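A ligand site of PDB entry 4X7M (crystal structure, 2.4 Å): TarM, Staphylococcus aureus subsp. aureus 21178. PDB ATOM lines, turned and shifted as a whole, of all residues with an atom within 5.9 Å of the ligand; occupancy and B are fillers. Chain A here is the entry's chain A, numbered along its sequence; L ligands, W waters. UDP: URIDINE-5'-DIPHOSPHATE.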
ATOM      1  N   GLY A  16      23.267  17.479   3.790  1.00  0.00           N
ATOM      2  CA  GLY A  16      24.413  16.632   3.503  1.00  0.00           C
ATOM      3  C   GLY A  16      24.693  16.368   2.030  1.00  0.00           C
ATOM      4  O   GLY A  16      23.822  16.540   1.183  1.00  0.00           O
ATOM      5  N   GLY A  17      25.932  15.954   1.745  1.00  0.00           N
ATOM      6  CA  GLY A  17      26.373  15.657   0.388  1.00  0.00           C
ATOM      7  C   GLY A  17      27.046  16.836  -0.276  1.00  0.00           C
ATOM      8  O   GLY A  17      28.266  16.805  -0.463  1.00  0.00           O
ATOM      9  N   MET A  18      26.247  17.865  -0.681  1.00  0.00           N
ATOM     10  CA  MET A  18      26.771  19.086  -1.313  1.00  0.00           C
ATOM     11  C   MET A  18      27.441  19.954  -0.247  1.00  0.00           C
ATOM     12  O   MET A  18      28.527  20.446  -0.512  1.00  0.00           O
ATOM     13  CB  MET A  18      25.670  19.850  -2.042  1.00  0.00           C
ATOM     14  CG  MET A  18      26.146  21.125  -2.684  1.00  0.00           C
ATOM     15  SD  MET A  18      24.915  22.030  -3.636  1.00  0.00           S
ATOM     16  CE  MET A  18      23.504  22.096  -2.490  1.00  0.00           C
ATOM     17  N   ILE A 324      25.257   1.962   2.602  1.00  0.00           N
ATOM     18  CA  ILE A 324      25.088   3.160   3.418  1.00  0.00           C
ATOM     19  C   ILE A 324      24.742   4.333   2.500  1.00  0.00           C
ATOM     20  O   ILE A 324      25.601   4.804   1.755  1.00  0.00           O
ATOM     21  CB  ILE A 324      26.312   3.490   4.335  1.00  0.00           C
ATOM     22  CG1 ILE A 324      26.840   2.263   5.076  1.00  0.00           C
ATOM     23  CG2 ILE A 324      25.965   4.633   5.326  1.00  0.00           C
ATOM     24  CD1 ILE A 324      28.187   2.452   5.770  1.00  0.00           C
ATOM     25  N   SER A 325      23.503   4.817   2.591  1.00  0.00           N
ATOM     26  CA  SER A 325      23.050   5.958   1.796  1.00  0.00           C
ATOM     27  C   SER A 325      21.788   6.554   2.414  1.00  0.00           C
ATOM     28  O   SER A 325      21.254   6.016   3.386  1.00  0.00           O
ATOM     29  CB  SER A 325      22.717   5.504   0.377  1.00  0.00           C
ATOM     30  OG  SER A 325      21.575   4.655   0.387  1.00  0.00           O
ATOM     31  N   ARG A 326      21.283   7.609   1.781  1.00  0.00           N
ATOM     32  CA  ARG A 326      19.975   8.169   2.097  1.00  0.00           C
ATOM     33  C   ARG A 326      18.986   7.227   1.365  1.00  0.00           C
ATOM     34  O   ARG A 326      19.172   6.931   0.178  1.00  0.00           O
ATOM     35  CB  ARG A 326      19.827   9.596   1.532  1.00  0.00           C
ATOM     36  CG  ARG A 326      20.811  10.638   2.101  1.00  0.00           C
ATOM     37  CD  ARG A 326      20.729  11.980   1.369  1.00  0.00           C
ATOM     38  NE  ARG A 326      21.059  11.842  -0.056  1.00  0.00           N
ATOM     39  CZ  ARG A 326      20.198  12.014  -1.063  1.00  0.00           C
ATOM     40  NH1 ARG A 326      18.945  12.378  -0.819  1.00  0.00           N
ATOM     41  NH2 ARG A 326      20.588  11.811  -2.313  1.00  0.00           N
ATOM     42  N   VAL A 328      16.563   6.936  -0.663  1.00  0.00           N
ATOM     43  CA  VAL A 328      15.840   7.708  -1.696  1.00  0.00           C
ATOM     44  C   VAL A 328      15.642   6.962  -3.012  1.00  0.00           C
ATOM     45  O   VAL A 328      16.390   6.018  -3.289  1.00  0.00           O
ATOM     46  CB  VAL A 328      16.463   9.112  -1.905  1.00  0.00           C
ATOM     47  CG1 VAL A 328      16.443   9.926  -0.614  1.00  0.00           C
ATOM     48  CG2 VAL A 328      17.873   9.056  -2.516  1.00  0.00           C
ATOM     49  N   LYS A 331      18.744   5.843  -5.548  1.00  0.00           N
ATOM     50  CA  LYS A 331      19.603   4.799  -4.961  1.00  0.00           C
ATOM     51  C   LYS A 331      19.168   3.400  -5.335  1.00  0.00           C
ATOM     52  O   LYS A 331      19.960   2.462  -5.237  1.00  0.00           O
ATOM     53  CB  LYS A 331      19.616   4.928  -3.422  1.00  0.00           C
ATOM     54  CG  LYS A 331      20.209   6.234  -2.917  1.00  0.00           C
ATOM     55  CD  LYS A 331      21.653   6.395  -3.315  1.00  0.00           C
ATOM     56  CE  LYS A 331      22.284   7.647  -2.783  1.00  0.00           C
ATOM     57  NZ  LYS A 331      23.651   7.815  -3.374  1.00  0.00           N
ATOM     58  N   TYR A 355      22.072   0.750   5.852  1.00  0.00           N
ATOM     59  CA  TYR A 355      22.065   1.924   6.727  1.00  0.00           C
ATOM     60  C   TYR A 355      21.481   3.107   6.012  1.00  0.00           C
ATOM     61  O   TYR A 355      21.650   3.254   4.778  1.00  0.00           O
ATOM     62  CB  TYR A 355      23.478   2.239   7.242  1.00  0.00           C
ATOM     63  CG  TYR A 355      23.977   1.224   8.239  1.00  0.00           C
ATOM     64  CD1 TYR A 355      24.602   0.059   7.811  1.00  0.00           C
ATOM     65  CD2 TYR A 355      23.770   1.402   9.609  1.00  0.00           C
ATOM     66  CE1 TYR A 355      25.033  -0.900   8.737  1.00  0.00           C
ATOM     67  CE2 TYR A 355      24.216   0.472  10.532  1.00  0.00           C
ATOM     68  CZ  TYR A 355      24.847  -0.684  10.096  1.00  0.00           C
ATOM     69  OH  TYR A 355      25.297  -1.614  10.996  1.00  0.00           O
ATOM     70  N   GLY A 356      20.784   3.927   6.781  1.00  0.00           N
ATOM     71  CA  GLY A 356      20.156   5.153   6.322  1.00  0.00           C
ATOM     72  C   GLY A 356      18.696   5.253   6.611  1.00  0.00           C
ATOM     73  O   GLY A 356      18.088   4.320   7.150  1.00  0.00           O
ATOM     74  N   GLU A 357      18.142   6.413   6.251  1.00  0.00           N
ATOM     75  CA  GLU A 357      16.721   6.761   6.327  1.00  0.00           C
ATOM     76  C   GLU A 357      16.247   7.633   5.163  1.00  0.00           C
ATOM     77  O   GLU A 357      17.085   8.267   4.491  1.00  0.00           O
ATOM     78  CB  GLU A 357      16.281   7.259   7.709  1.00  0.00           C
ATOM     79  CG  GLU A 357      17.041   8.410   8.305  1.00  0.00           C
ATOM     80  CD  GLU A 357      17.018   8.342   9.820  1.00  0.00           C
ATOM     81  OE1 GLU A 357      16.646   7.268  10.364  1.00  0.00           O
ATOM     82  OE2 GLU A 357      17.439   9.330  10.457  1.00  0.00           O
ATOM     83  N   GLY A 381      18.870   1.526  10.022  1.00  0.00           N
ATOM     84  CA  GLY A 381      18.603   2.933  10.299  1.00  0.00           C
ATOM     85  C   GLY A 381      19.803   3.817  10.038  1.00  0.00           C
ATOM     86  O   GLY A 381      20.839   3.330   9.542  1.00  0.00           O
ATOM     87  N   TYR A 382      19.706   5.119  10.407  1.00  0.00           N
ATOM     88  CA  TYR A 382      20.774   6.105  10.234  1.00  0.00           C
ATOM     89  C   TYR A 382      22.018   5.811  11.078  1.00  0.00           C
ATOM     90  O   TYR A 382      21.921   5.287  12.189  1.00  0.00           O
ATOM     91  CB  TYR A 382      20.258   7.532  10.528  1.00  0.00           C
ATOM     92  CG  TYR A 382      21.159   8.621   9.980  1.00  0.00           C
ATOM     93  CD1 TYR A 382      21.146   8.964   8.630  1.00  0.00           C
ATOM     94  CD2 TYR A 382      22.073   9.278  10.810  1.00  0.00           C
ATOM     95  CE1 TYR A 382      22.010   9.936   8.124  1.00  0.00           C
ATOM     96  CE2 TYR A 382      22.945  10.240  10.310  1.00  0.00           C
ATOM     97  CZ  TYR A 382      22.907  10.564   8.957  1.00  0.00           C
ATOM     98  OH  TYR A 382      23.781  11.505   8.470  1.00  0.00           O
ATOM     99  N   THR A 383      23.212   6.134  10.534  1.00  0.00           N
ATOM    100  CA  THR A 383      24.486   5.988  11.223  1.00  0.00           C
ATOM    101  C   THR A 383      25.274   7.298  11.245  1.00  0.00           C
ATOM    102  O   THR A 383      25.376   7.982  10.202  1.00  0.00           O
ATOM    103  CB  THR A 383      25.292   4.768  10.748  1.00  0.00           C
ATOM    104  OG1 THR A 383      26.391   4.586  11.647  1.00  0.00           O
ATOM    105  CG2 THR A 383      25.811   4.896   9.289  1.00  0.00           C
ATOM    106  N   THR A 384      25.807   7.645  12.418  1.00  0.00           N
ATOM    107  CA  THR A 384      26.616   8.852  12.615  1.00  0.00           C
ATOM    108  C   THR A 384      28.084   8.540  12.305  1.00  0.00           C
ATOM    109  O   THR A 384      28.877   9.458  12.066  1.00  0.00           O
ATOM    110  CB  THR A 384      26.422   9.390  14.046  1.00  0.00           C
ATOM    111  OG1 THR A 384      26.724   8.351  14.976  1.00  0.00           O
ATOM    112  CG2 THR A 384      25.010   9.908  14.297  1.00  0.00           C
ATOM    113  N   THR A 385      28.432   7.237  12.302  1.00  0.00           N
ATOM    114  CA  THR A 385      29.776   6.695  12.079  1.00  0.00           C
ATOM    115  C   THR A 385      29.780   5.661  10.933  1.00  0.00           C
ATOM    116  O   THR A 385      29.996   4.469  11.220  1.00  0.00           O
ATOM    117  CB  THR A 385      30.349   6.115  13.386  1.00  0.00           C
ATOM    118  OG1 THR A 385      29.426   5.168  13.949  1.00  0.00           O
ATOM    119  CG2 THR A 385      30.707   7.199  14.407  1.00  0.00           C
ATOM    120  N   PRO A 386      29.583   6.069   9.651  1.00  0.00           N
ATOM    121  CA  PRO A 386      29.629   5.072   8.554  1.00  0.00           C
ATOM    122  C   PRO A 386      30.959   4.350   8.404  1.00  0.00           C
ATOM    123  O   PRO A 386      31.000   3.203   7.919  1.00  0.00           O
ATOM    124  CB  PRO A 386      29.293   5.903   7.303  1.00  0.00           C
ATOM    125  CG  PRO A 386      29.569   7.305   7.681  1.00  0.00           C
ATOM    126  CD  PRO A 386      29.305   7.426   9.149  1.00  0.00           C
ATOM    127  N   GLU A 403      24.160   9.480 -10.226  1.00  0.00           N
ATOM    128  CA  GLU A 403      25.229   9.954  -9.346  1.00  0.00           C
ATOM    129  C   GLU A 403      26.087  11.007 -10.051  1.00  0.00           C
ATOM    130  O   GLU A 403      26.167  11.020 -11.276  1.00  0.00           O
ATOM    131  CB  GLU A 403      26.108   8.747  -8.975  1.00  0.00           C
ATOM    132  CG  GLU A 403      26.437   8.599  -7.515  1.00  0.00           C
ATOM    133  CD  GLU A 403      25.316   8.140  -6.606  1.00  0.00           C
ATOM    134  OE1 GLU A 403      24.806   7.018  -6.828  1.00  0.00           O
ATOM    135  OE2 GLU A 403      25.004   8.858  -5.630  1.00  0.00           O
ATOM    136  N   GLN A 405      29.337  11.400  -8.674  1.00  0.00           N
ATOM    137  CA  GLN A 405      30.547  10.668  -8.365  1.00  0.00           C
ATOM    138  C   GLN A 405      30.271   9.426  -7.475  1.00  0.00           C
ATOM    139  O   GLN A 405      30.713   8.326  -7.834  1.00  0.00           O
ATOM    140  CB  GLN A 405      31.558  11.598  -7.724  1.00  0.00           C
ATOM    141  CG  GLN A 405      32.958  11.020  -7.670  1.00  0.00           C
ATOM    142  CD  GLN A 405      33.934  12.003  -7.115  1.00  0.00           C
ATOM    143  OE1 GLN A 405      33.588  12.955  -6.389  1.00  0.00           O
ATOM    144  NE2 GLN A 405      35.190  11.829  -7.486  1.00  0.00           N
ATOM    145  N   GLY A 406      29.592   9.593  -6.338  1.00  0.00           N
ATOM    146  CA  GLY A 406      29.288   8.444  -5.484  1.00  0.00           C
ATOM    147  C   GLY A 406      30.273   8.242  -4.359  1.00  0.00           C
ATOM    148  O   GLY A 406      31.022   7.267  -4.347  1.00  0.00           O
ATOM    149  N   LEU A 407      30.245   9.177  -3.426  1.00  0.00           N
ATOM    150  CA  LEU A 407      31.110   9.266  -2.263  1.00  0.00           C
ATOM    151  C   LEU A 407      31.115   8.101  -1.280  1.00  0.00           C
ATOM    152  O   LEU A 407      32.177   7.803  -0.744  1.00  0.00           O
ATOM    153  CB  LEU A 407      30.893  10.598  -1.557  1.00  0.00           C
ATOM    154  CG  LEU A 407      31.430  11.858  -2.278  1.00  0.00           C
ATOM    155  CD1 LEU A 407      31.414  13.064  -1.327  1.00  0.00           C
ATOM    156  CD2 LEU A 407      32.852  11.640  -2.872  1.00  0.00           C
ATOM    157  N   SER A 408      29.968   7.444  -1.033  1.00  0.00           N
ATOM    158  CA  SER A 408      29.846   6.249  -0.154  1.00  0.00           C
ATOM    159  C   SER A 408      30.684   5.086  -0.707  1.00  0.00           C
ATOM    160  O   SER A 408      31.275   4.335   0.073  1.00  0.00           O
ATOM    161  CB  SER A 408      28.394   5.797  -0.020  1.00  0.00           C
ATOM    162  OG  SER A 408      27.731   6.474   1.029  1.00  0.00           O
ATOM    163  N   MET A 409      30.712   4.954  -2.052  1.00  0.00           N
ATOM    164  CA  MET A 409      31.440   3.941  -2.803  1.00  0.00           C
ATOM    165  C   MET A 409      32.924   4.219  -2.621  1.00  0.00           C
ATOM    166  O   MET A 409      33.664   3.315  -2.238  1.00  0.00           O
ATOM    167  CB  MET A 409      31.051   3.973  -4.296  1.00  0.00           C
ATOM    168  CG  MET A 409      29.656   3.406  -4.596  1.00  0.00           C
ATOM    169  SD  MET A 409      29.124   3.691  -6.314  1.00  0.00           S
ATOM    170  CE  MET A 409      30.079   2.699  -7.062  1.00  0.00           C
ATOM    171  N   GLU A 411      34.241   6.016  -0.136  1.00  0.00           N
ATOM    172  CA  GLU A 411      34.436   5.799   1.301  1.00  0.00           C
ATOM    173  C   GLU A 411      34.681   4.334   1.620  1.00  0.00           C
ATOM    174  O   GLU A 411      35.591   4.018   2.369  1.00  0.00           O
ATOM    175  CB  GLU A 411      33.223   6.291   2.087  1.00  0.00           C
ATOM    176  CG  GLU A 411      33.194   7.778   2.358  1.00  0.00           C
ATOM    177  CD  GLU A 411      31.846   8.311   2.806  1.00  0.00           C
ATOM    178  OE1 GLU A 411      31.141   7.587   3.557  1.00  0.00           O
ATOM    179  OE2 GLU A 411      31.476   9.425   2.376  1.00  0.00           O
HETATM  180  N1  UDP L   1      25.538   8.621   5.349  1.00  0.00           N
HETATM  181  C2  UDP L   1      25.779   8.401   6.697  1.00  0.00           C
HETATM  182  N3  UDP L   1      24.855   7.604   7.334  1.00  0.00           N
HETATM  183  C4  UDP L   1      23.682   7.089   6.793  1.00  0.00           C
HETATM  184  C5  UDP L   1      23.467   7.428   5.421  1.00  0.00           C
HETATM  185  C6  UDP L   1      24.384   8.145   4.747  1.00  0.00           C
HETATM  186  O2  UDP L   1      26.689   8.947   7.316  1.00  0.00           O
HETATM  187  O4  UDP L   1      22.939   6.388   7.495  1.00  0.00           O
HETATM  188  C1' UDP L   1      26.574   9.329   4.528  1.00  0.00           C
HETATM  189  C2' UDP L   1      27.664   8.426   3.933  1.00  0.00           C
HETATM  190  O2' UDP L   1      28.704   8.109   4.849  1.00  0.00           O
HETATM  191  C3' UDP L   1      28.189   9.326   2.819  1.00  0.00           C
HETATM  192  C4' UDP L   1      26.926  10.012   2.311  1.00  0.00           C
HETATM  193  O4' UDP L   1      25.951   9.902   3.390  1.00  0.00           O
HETATM  194  O3' UDP L   1      29.067  10.337   3.308  1.00  0.00           O
HETATM  195  C5' UDP L   1      26.365   9.477   1.011  1.00  0.00           C
HETATM  196  O5' UDP L   1      27.207   9.809  -0.131  1.00  0.00           O
HETATM  197  PA  UDP L   1      26.800   9.552  -1.669  1.00  0.00           P
HETATM  198  O1A UDP L   1      26.972   8.123  -2.041  1.00  0.00           O
HETATM  199  O2A UDP L   1      27.606  10.429  -2.648  1.00  0.00           O
HETATM  200  O3A UDP L   1      25.289   9.917  -1.819  1.00  0.00           O
HETATM  201  PB  UDP L   1      24.361  11.208  -1.570  1.00  0.00           P
HETATM  202  O1B UDP L   1      23.239  11.090  -2.599  1.00  0.00           O
HETATM  203  O2B UDP L   1      23.845  11.181  -0.138  1.00  0.00           O
HETATM  204  O3B UDP L   1      25.112  12.451  -1.794  1.00  0.00           O
HETATM  205  O   HOH W   1      23.220  10.701  -5.523  1.00  0.00           O
HETATM  206  O   HOH W   2      29.256  12.319  -4.758  1.00  0.00           O
HETATM  207  O   HOH W   3      27.670  13.303  -1.830  1.00  0.00           O
HETATM  208  O   HOH W   4      26.674  10.937  -5.746  1.00  0.00           O
HETATM  209  O   HOH W   5      23.425   8.827   0.372  1.00  0.00           O
HETATM  210  O   HOH W   6      24.682  12.305   2.227  1.00  0.00           O
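The side-chain carboxylate of Glu 411 is in hydrogen-bond range of an oxygen (O3') of the ligand (2.7 Å). The guanidinium group of Arg 326 is in salt-bridge range of an oxygen (O1B) of the ligand (2.8 Å). The backbone NH of Thr 383 sits at hydrogen-bond distance from an oxygen (O4) of the ligand (3.1 Å). A nitrogen (N3) of the ligand sits at hydrogen-bond distance from the backbone carbonyl oxygen (O) of Thr 383 (2.9 Å). N of Leu 407 lies within hydrogen-bond range of O2A of the ligand (3.0 Å). The side-chain amino group (NZ) of Lys 331 lies within salt-bridge range of an oxygen (O1B) of the ligand (3.4 Å). An oxygen (O1A) of the ligand sits at hydrogen-bond distance from the backbone NH (N) of Ser 408 (3.2 Å). The backbone NH (N) of Gly 356 lies close to an oxygen (O4) of the ligand (3.3 Å).
OG1 of Thr 383 lies close to N of Thr 385 (3.4 Å). NZ of Lys 331 is in salt-bridge range of OE2 of Glu 403 (2.8 Å). O of Ile 324 lies within hydrogen-bond range of OG of Ser 408. O of Gly 381 is in hydrogen-bond range of N of Gly 356 (2.8 Å). O of Tyr 355 sits at hydrogen-bond distance from N of Ser 325, 3.3 Å away.
Ile 324 touches the ligand. O of Ser 325 touches C5 of the ligand (3.3 Å). Tyr 355 touches the ligand. CD1 of Tyr 382 touches O4 of the ligand, at 3.3 Å. CG of Pro 386 touches O2' of the ligand, 3.1 Å away. Glu 403 touches the ligand. Gly 406 touches the ligand. Hydrophobic or aromatic side chains that line the ligand: Ile 324, Tyr 382, Pro 386 and Leu 407. Within 4 Å of the ligand: Ile 324, Ser 325, Arg 326, Lys 331, Tyr 355, Gly 356, Tyr 382, Thr 383, Pro 386, Glu 403, Gly 406, Leu 407, Ser 408 and Glu 411.
Water W5 lies within hydrogen-bond range of an oxygen (O2B) of the ligand and the backbone NH (N) of Arg 326. Water W1 lies within hydrogen-bond range of the side-chain carboxylate (OE2) of Glu 403 (2.6 Å) and an oxygen (O1B) of the ligand (2.9 Å). Water W4 lies within hydrogen-bond range of OE2 of Glu 403 (2.7 Å), N of Gly 406 (3.3 Å) and O2A of the ligand (3.3 Å). Water W2 bridges N of Gly 406 (3.2 Å) and O2A of the ligand (3.3 Å).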
